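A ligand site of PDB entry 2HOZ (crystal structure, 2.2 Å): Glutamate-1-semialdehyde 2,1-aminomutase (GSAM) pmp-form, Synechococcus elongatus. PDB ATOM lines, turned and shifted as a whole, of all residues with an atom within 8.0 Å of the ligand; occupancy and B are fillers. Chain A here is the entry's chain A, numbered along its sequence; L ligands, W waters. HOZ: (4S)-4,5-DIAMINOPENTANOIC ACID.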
ATOM      1  N   GLU A 146       6.655  -8.309 -14.711  1.00  0.00           N
ATOM      2  CA  GLU A 146       5.373  -8.286 -14.016  1.00  0.00           C
ATOM      3  C   GLU A 146       4.417  -9.202 -14.770  1.00  0.00           C
ATOM      4  O   GLU A 146       4.301  -9.107 -15.996  1.00  0.00           O
ATOM      5  CB  GLU A 146       4.806  -6.868 -14.002  1.00  0.00           C
ATOM      6  CG  GLU A 146       3.580  -6.726 -13.123  1.00  0.00           C
ATOM      7  CD  GLU A 146       2.888  -5.390 -13.316  1.00  0.00           C
ATOM      8  OE1 GLU A 146       2.034  -5.037 -12.470  1.00  0.00           O
ATOM      9  OE2 GLU A 146       3.179  -4.711 -14.318  1.00  0.00           O
ATOM     10  N   GLY A 147       3.741 -10.080 -14.043  1.00  0.00           N
ATOM     11  CA  GLY A 147       2.816 -10.992 -14.702  1.00  0.00           C
ATOM     12  C   GLY A 147       3.399 -12.389 -14.834  1.00  0.00           C
ATOM     13  O   GLY A 147       2.663 -13.348 -15.056  1.00  0.00           O
ATOM     14  N   ALA A 160       5.024  -5.529  -8.019  1.00  0.00           N
ATOM     15  CA  ALA A 160       5.399  -5.075  -9.345  1.00  0.00           C
ATOM     16  C   ALA A 160       4.406  -4.025  -9.829  1.00  0.00           C
ATOM     17  O   ALA A 160       3.351  -3.825  -9.214  1.00  0.00           O
ATOM     18  CB  ALA A 160       5.420  -6.246 -10.316  1.00  0.00           C
ATOM     19  N   GLY A 161       4.750  -3.367 -10.920  1.00  0.00           N
ATOM     20  CA  GLY A 161       3.888  -2.324 -11.459  1.00  0.00           C
ATOM     21  C   GLY A 161       4.605  -0.992 -11.458  1.00  0.00           C
ATOM     22  O   GLY A 161       5.614  -0.824 -10.759  1.00  0.00           O
ATOM     23  N   SER A 162       4.098  -0.042 -12.221  1.00  0.00           N
ATOM     24  CA  SER A 162       4.693   1.289 -12.304  1.00  0.00           C
ATOM     25  C   SER A 162       4.813   1.910 -10.920  1.00  0.00           C
ATOM     26  O   SER A 162       3.871   1.886 -10.138  1.00  0.00           O
ATOM     27  CB  SER A 162       3.823   2.193 -13.181  1.00  0.00           C
ATOM     28  OG  SER A 162       3.466   1.540 -14.390  1.00  0.00           O
ATOM     29  N   GLY A 163       5.989   2.451 -10.617  1.00  0.00           N
ATOM     30  CA  GLY A 163       6.183   3.075  -9.317  1.00  0.00           C
ATOM     31  C   GLY A 163       6.930   2.236  -8.294  1.00  0.00           C
ATOM     32  O   GLY A 163       7.452   2.785  -7.338  1.00  0.00           O
ATOM     33  N   VAL A 164       6.987   0.921  -8.484  1.00  0.00           N
ATOM     34  CA  VAL A 164       7.703   0.072  -7.529  1.00  0.00           C
ATOM     35  C   VAL A 164       8.623  -0.945  -8.217  1.00  0.00           C
ATOM     36  O   VAL A 164       9.125  -1.874  -7.580  1.00  0.00           O
ATOM     37  CB  VAL A 164       6.739  -0.709  -6.603  1.00  0.00           C
ATOM     38  CG1 VAL A 164       5.876   0.276  -5.812  1.00  0.00           C
ATOM     39  CG2 VAL A 164       5.860  -1.657  -7.419  1.00  0.00           C
ATOM     40  N   ALA A 165       8.833  -0.747  -9.513  1.00  0.00           N
ATOM     41  CA  ALA A 165       9.666  -1.631 -10.329  1.00  0.00           C
ATOM     42  C   ALA A 165      11.048  -1.900  -9.749  1.00  0.00           C
ATOM     43  O   ALA A 165      11.598  -2.989  -9.922  1.00  0.00           O
ATOM     44  CB  ALA A 165       9.813  -1.040 -11.728  1.00  0.00           C
ATOM     45  N   THR A 185      11.764  -5.521 -11.463  1.00  0.00           N
ATOM     46  CA  THR A 185      10.718  -5.942 -12.381  1.00  0.00           C
ATOM     47  C   THR A 185      10.562  -4.964 -13.517  1.00  0.00           C
ATOM     48  O   THR A 185      10.927  -3.783 -13.413  1.00  0.00           O
ATOM     49  CB  THR A 185       9.357  -6.092 -11.673  1.00  0.00           C
ATOM     50  OG1 THR A 185       8.949  -4.821 -11.149  1.00  0.00           O
ATOM     51  CG2 THR A 185       9.443  -7.132 -10.551  1.00  0.00           C
ATOM     52  N   THR A 186       9.999  -5.459 -14.607  1.00  0.00           N
ATOM     53  CA  THR A 186       9.778  -4.666 -15.804  1.00  0.00           C
ATOM     54  C   THR A 186       8.550  -5.204 -16.512  1.00  0.00           C
ATOM     55  O   THR A 186       8.171  -6.357 -16.329  1.00  0.00           O
ATOM     56  CB  THR A 186      10.982  -4.744 -16.743  1.00  0.00           C
ATOM     57  OG1 THR A 186      10.586  -4.412 -18.073  1.00  0.00           O
ATOM     58  CG2 THR A 186      11.570  -6.143 -16.724  1.00  0.00           C
ATOM     59  N   PRO A 187       7.888  -4.363 -17.330  1.00  0.00           N
ATOM     60  CA  PRO A 187       6.694  -4.803 -18.047  1.00  0.00           C
ATOM     61  C   PRO A 187       7.072  -5.840 -19.095  1.00  0.00           C
ATOM     62  O   PRO A 187       8.091  -5.697 -19.771  1.00  0.00           O
ATOM     63  CB  PRO A 187       6.186  -3.511 -18.698  1.00  0.00           C
ATOM     64  CG  PRO A 187       6.776  -2.422 -17.834  1.00  0.00           C
ATOM     65  CD  PRO A 187       8.145  -2.928 -17.547  1.00  0.00           C
ATOM     66  N   TYR A 188       6.276  -6.885 -19.227  1.00  0.00           N
ATOM     67  CA  TYR A 188       6.571  -7.896 -20.237  1.00  0.00           C
ATOM     68  C   TYR A 188       6.511  -7.196 -21.599  1.00  0.00           C
ATOM     69  O   TYR A 188       5.818  -6.193 -21.750  1.00  0.00           O
ATOM     70  CB  TYR A 188       5.551  -9.033 -20.178  1.00  0.00           C
ATOM     71  CG  TYR A 188       5.988 -10.254 -20.944  1.00  0.00           C
ATOM     72  CD1 TYR A 188       6.897 -11.157 -20.397  1.00  0.00           C
ATOM     73  CD2 TYR A 188       5.503 -10.502 -22.228  1.00  0.00           C
ATOM     74  CE1 TYR A 188       7.325 -12.274 -21.106  1.00  0.00           C
ATOM     75  CE2 TYR A 188       5.922 -11.620 -22.951  1.00  0.00           C
ATOM     76  CZ  TYR A 188       6.831 -12.505 -22.380  1.00  0.00           C
ATOM     77  OH  TYR A 188       7.241 -13.608 -23.079  1.00  0.00           O
ATOM     78  N   ASN A 189       7.238  -7.725 -22.584  1.00  0.00           N
ATOM     79  CA  ASN A 189       7.226  -7.120 -23.906  1.00  0.00           C
ATOM     80  C   ASN A 189       7.708  -5.671 -23.933  1.00  0.00           C
ATOM     81  O   ASN A 189       7.327  -4.902 -24.808  1.00  0.00           O
ATOM     82  CB  ASN A 189       5.821  -7.189 -24.511  1.00  0.00           C
ATOM     83  CG  ASN A 189       5.578  -8.469 -25.259  1.00  0.00           C
ATOM     84  OD1 ASN A 189       4.441  -8.961 -25.342  1.00  0.00           O
ATOM     85  ND2 ASN A 189       6.634  -9.034 -25.824  1.00  0.00           N
ATOM     86  N   ASP A 190       8.550  -5.299 -22.967  1.00  0.00           N
ATOM     87  CA  ASP A 190       9.066  -3.931 -22.893  1.00  0.00           C
ATOM     88  C   ASP A 190      10.594  -3.938 -22.848  1.00  0.00           C
ATOM     89  O   ASP A 190      11.190  -3.908 -21.771  1.00  0.00           O
ATOM     90  CB  ASP A 190       8.523  -3.248 -21.633  1.00  0.00           C
ATOM     91  CG  ASP A 190       8.680  -1.734 -21.678  1.00  0.00           C
ATOM     92  OD1 ASP A 190       9.733  -1.248 -22.155  1.00  0.00           O
ATOM     93  OD2 ASP A 190       7.756  -1.039 -21.228  1.00  0.00           O
ATOM     94  N   ALA A 193      12.352  -0.992 -21.165  1.00  0.00           N
ATOM     95  CA  ALA A 193      12.209  -1.082 -19.723  1.00  0.00           C
ATOM     96  C   ALA A 193      13.369  -1.889 -19.150  1.00  0.00           C
ATOM     97  O   ALA A 193      13.873  -1.576 -18.083  1.00  0.00           O
ATOM     98  CB  ALA A 193      10.894  -1.763 -19.365  1.00  0.00           C
ATOM     99  N   HIS A 372      -0.559  -7.340 -24.368  1.00  0.00           N
ATOM    100  CA  HIS A 372       0.886  -7.467 -24.566  1.00  0.00           C
ATOM    101  C   HIS A 372       1.626  -7.629 -23.241  1.00  0.00           C
ATOM    102  O   HIS A 372       2.786  -8.041 -23.216  1.00  0.00           O
ATOM    103  CB  HIS A 372       1.438  -6.234 -25.297  1.00  0.00           C
ATOM    104  CG  HIS A 372       0.993  -6.114 -26.715  1.00  0.00           C
ATOM    105  ND1 HIS A 372      -0.318  -5.867 -27.081  1.00  0.00           N
ATOM    106  CD2 HIS A 372       1.693  -6.212 -27.875  1.00  0.00           C
ATOM    107  CE1 HIS A 372      -0.405  -5.813 -28.393  1.00  0.00           C
ATOM    108  NE2 HIS A 372       0.801  -6.010 -28.901  1.00  0.00           N
ATOM    109  N   ASN A 373       0.958  -7.292 -22.140  1.00  0.00           N
ATOM    110  CA  ASN A 373       1.576  -7.375 -20.825  1.00  0.00           C
ATOM    111  C   ASN A 373       0.544  -7.580 -19.721  1.00  0.00           C
ATOM    112  O   ASN A 373      -0.643  -7.714 -19.979  1.00  0.00           O
ATOM    113  CB  ASN A 373       2.360  -6.092 -20.558  1.00  0.00           C
ATOM    114  CG  ASN A 373       1.522  -4.849 -20.753  1.00  0.00           C
ATOM    115  OD1 ASN A 373       0.446  -4.717 -20.167  1.00  0.00           O
ATOM    116  ND2 ASN A 373       2.014  -3.927 -21.577  1.00  0.00           N
ATOM    117  N   TYR A 374       1.017  -7.590 -18.482  1.00  0.00           N
ATOM    118  CA  TYR A 374       0.123  -7.791 -17.352  1.00  0.00           C
ATOM    119  C   TYR A 374      -0.862  -6.634 -17.194  1.00  0.00           C
ATOM    120  O   TYR A 374      -2.021  -6.844 -16.852  1.00  0.00           O
ATOM    121  CB  TYR A 374       0.915  -7.962 -16.064  1.00  0.00           C
ATOM    122  CG  TYR A 374       0.045  -8.213 -14.856  1.00  0.00           C
ATOM    123  CD1 TYR A 374      -0.788  -9.328 -14.788  1.00  0.00           C
ATOM    124  CD2 TYR A 374       0.053  -7.332 -13.785  1.00  0.00           C
ATOM    125  CE1 TYR A 374      -1.594  -9.545 -13.687  1.00  0.00           C
ATOM    126  CE2 TYR A 374      -0.744  -7.549 -12.669  1.00  0.00           C
ATOM    127  CZ  TYR A 374      -1.576  -8.658 -12.628  1.00  0.00           C
ATOM    128  OH  TYR A 374      -2.384  -8.868 -11.533  1.00  0.00           O
ATOM    129  N   GLU A 375      -0.397  -5.414 -17.432  1.00  0.00           N
ATOM    130  CA  GLU A 375      -1.263  -4.246 -17.297  1.00  0.00           C
ATOM    131  C   GLU A 375      -2.459  -4.400 -18.237  1.00  0.00           C
ATOM    132  O   GLU A 375      -3.593  -4.130 -17.857  1.00  0.00           O
ATOM    133  CB  GLU A 375      -0.514  -2.949 -17.620  1.00  0.00           C
ATOM    134  CG  GLU A 375      -1.301  -1.698 -17.256  1.00  0.00           C
ATOM    135  CD  GLU A 375      -0.682  -0.420 -17.803  1.00  0.00           C
ATOM    136  OE1 GLU A 375      -1.149   0.675 -17.417  1.00  0.00           O
ATOM    137  OE2 GLU A 375       0.251  -0.511 -18.630  1.00  0.00           O
ATOM    138  N   ASP A 376      -2.199  -4.825 -19.469  1.00  0.00           N
ATOM    139  CA  ASP A 376      -3.274  -5.020 -20.435  1.00  0.00           C
ATOM    140  C   ASP A 376      -4.210  -6.124 -19.920  1.00  0.00           C
ATOM    141  O   ASP A 376      -5.432  -5.972 -19.934  1.00  0.00           O
ATOM    142  CB  ASP A 376      -2.739  -5.431 -21.814  1.00  0.00           C
ATOM    143  CG  ASP A 376      -1.863  -4.358 -22.446  1.00  0.00           C
ATOM    144  OD1 ASP A 376      -2.015  -3.173 -22.090  1.00  0.00           O
ATOM    145  OD2 ASP A 376      -1.043  -4.709 -23.306  1.00  0.00           O
ATOM    146  N   LYS A 378      -4.791  -7.056 -16.929  1.00  0.00           N
ATOM    147  CA  LYS A 378      -5.566  -6.561 -15.792  1.00  0.00           C
ATOM    148  C   LYS A 378      -6.814  -5.765 -16.147  1.00  0.00           C
ATOM    149  O   LYS A 378      -7.571  -5.364 -15.267  1.00  0.00           O
ATOM    150  CB  LYS A 378      -4.695  -5.701 -14.865  1.00  0.00           C
ATOM    151  CG  LYS A 378      -3.923  -6.499 -13.832  1.00  0.00           C
ATOM    152  CD  LYS A 378      -3.384  -5.580 -12.737  1.00  0.00           C
ATOM    153  CE  LYS A 378      -2.386  -4.562 -13.274  1.00  0.00           C
ATOM    154  NZ  LYS A 378      -1.814  -3.715 -12.185  1.00  0.00           N
HETATM  155  N   HOZ L   1       4.488  -0.117 -16.488  1.00  0.00           N
HETATM  156  CA  HOZ L   1       3.774  -1.400 -16.702  1.00  0.00           C
HETATM  157  C   HOZ L   1       2.882  -1.563 -17.938  1.00  0.00           C
HETATM  158  N1  HOZ L   1       3.139  -2.718 -18.826  1.00  0.00           N
HETATM  159  CB  HOZ L   1       3.044  -1.777 -15.364  1.00  0.00           C
HETATM  160  CG  HOZ L   1       1.618  -1.221 -15.087  1.00  0.00           C
HETATM  161  CD  HOZ L   1       1.066  -1.669 -13.772  1.00  0.00           C
HETATM  162  OE1 HOZ L   1       0.656  -2.853 -13.669  1.00  0.00           O
HETATM  163  OE2 HOZ L   1       1.019  -0.853 -12.831  1.00  0.00           O
HETATM  164  O   HOH W   1      -0.132  -1.923 -10.274  1.00  0.00           O
HETATM  165  O   HOH W   2       4.819  -1.343 -21.226  1.00  0.00           O
HETATM  166  O   HOH W   3       2.537  -4.822 -16.820  1.00  0.00           O
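OE2 of the ligand lies within hydrogen-bond range of N of Ser 162 (3.2 Å).
OE1 of Glu 146 sits close to OE1 of the ligand (2.8 Å).
OG of Ser 162 lies within hydrogen-bond range of N of the ligand.
An oxygen (OE1) of the ligand is in salt-bridge range of the side-chain amino group of Lys 378 (3.0 Å).
ND2 of Asn 373 sits close to N1 of the ligand (3.2 Å).
The side-chain carboxylate (OE2) of Glu 375 lies within salt-bridge range of a nitrogen (N1) of the ligand (3.6 Å).
The side-chain amide oxygen (OD1) of Asn 373 lies within hydrogen-bond range of the backbone NH (N) of Glu 375 (2.9 Å).
The backbone carbonyl oxygen (O) of Thr 186 lies within hydrogen-bond range of the backbone NH (N) of Glu 146, at 3.0 Å.
The side-chain amide oxygen (OD1) of Asn 373 is in hydrogen-bond range of the backbone NH (N) of Asp 376.
Residues that only touch the ligand: Pro 187 (3.2 Å) and Gly 161 (3.5 Å).
Hydrophobic or aromatic side chains that line the ligand: Pro 187.
Seven residues have an atom within 4 Å of the ligand: Glu 146, Gly 161, Ser 162, Pro 187, Asn 373, Glu 375 and Lys 378.
Along chain A the residues within 4 Å of the ligand span positions 146 to 378.
Water W3 lies within hydrogen-bond range of the side-chain carboxylate of Glu 146 (2.6 Å), a nitrogen (N1) of the ligand (3.0 Å) and the backbone NH of Glu 375 (3.1 Å).
Water W1 bridges OE2 of the ligand (3.0 Å) and NZ of Lys 378 (3.1 Å).
Water W2 bridges OD2 of Asp 190 (3.0 Å) and N1 of the ligand (3.2 Å).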
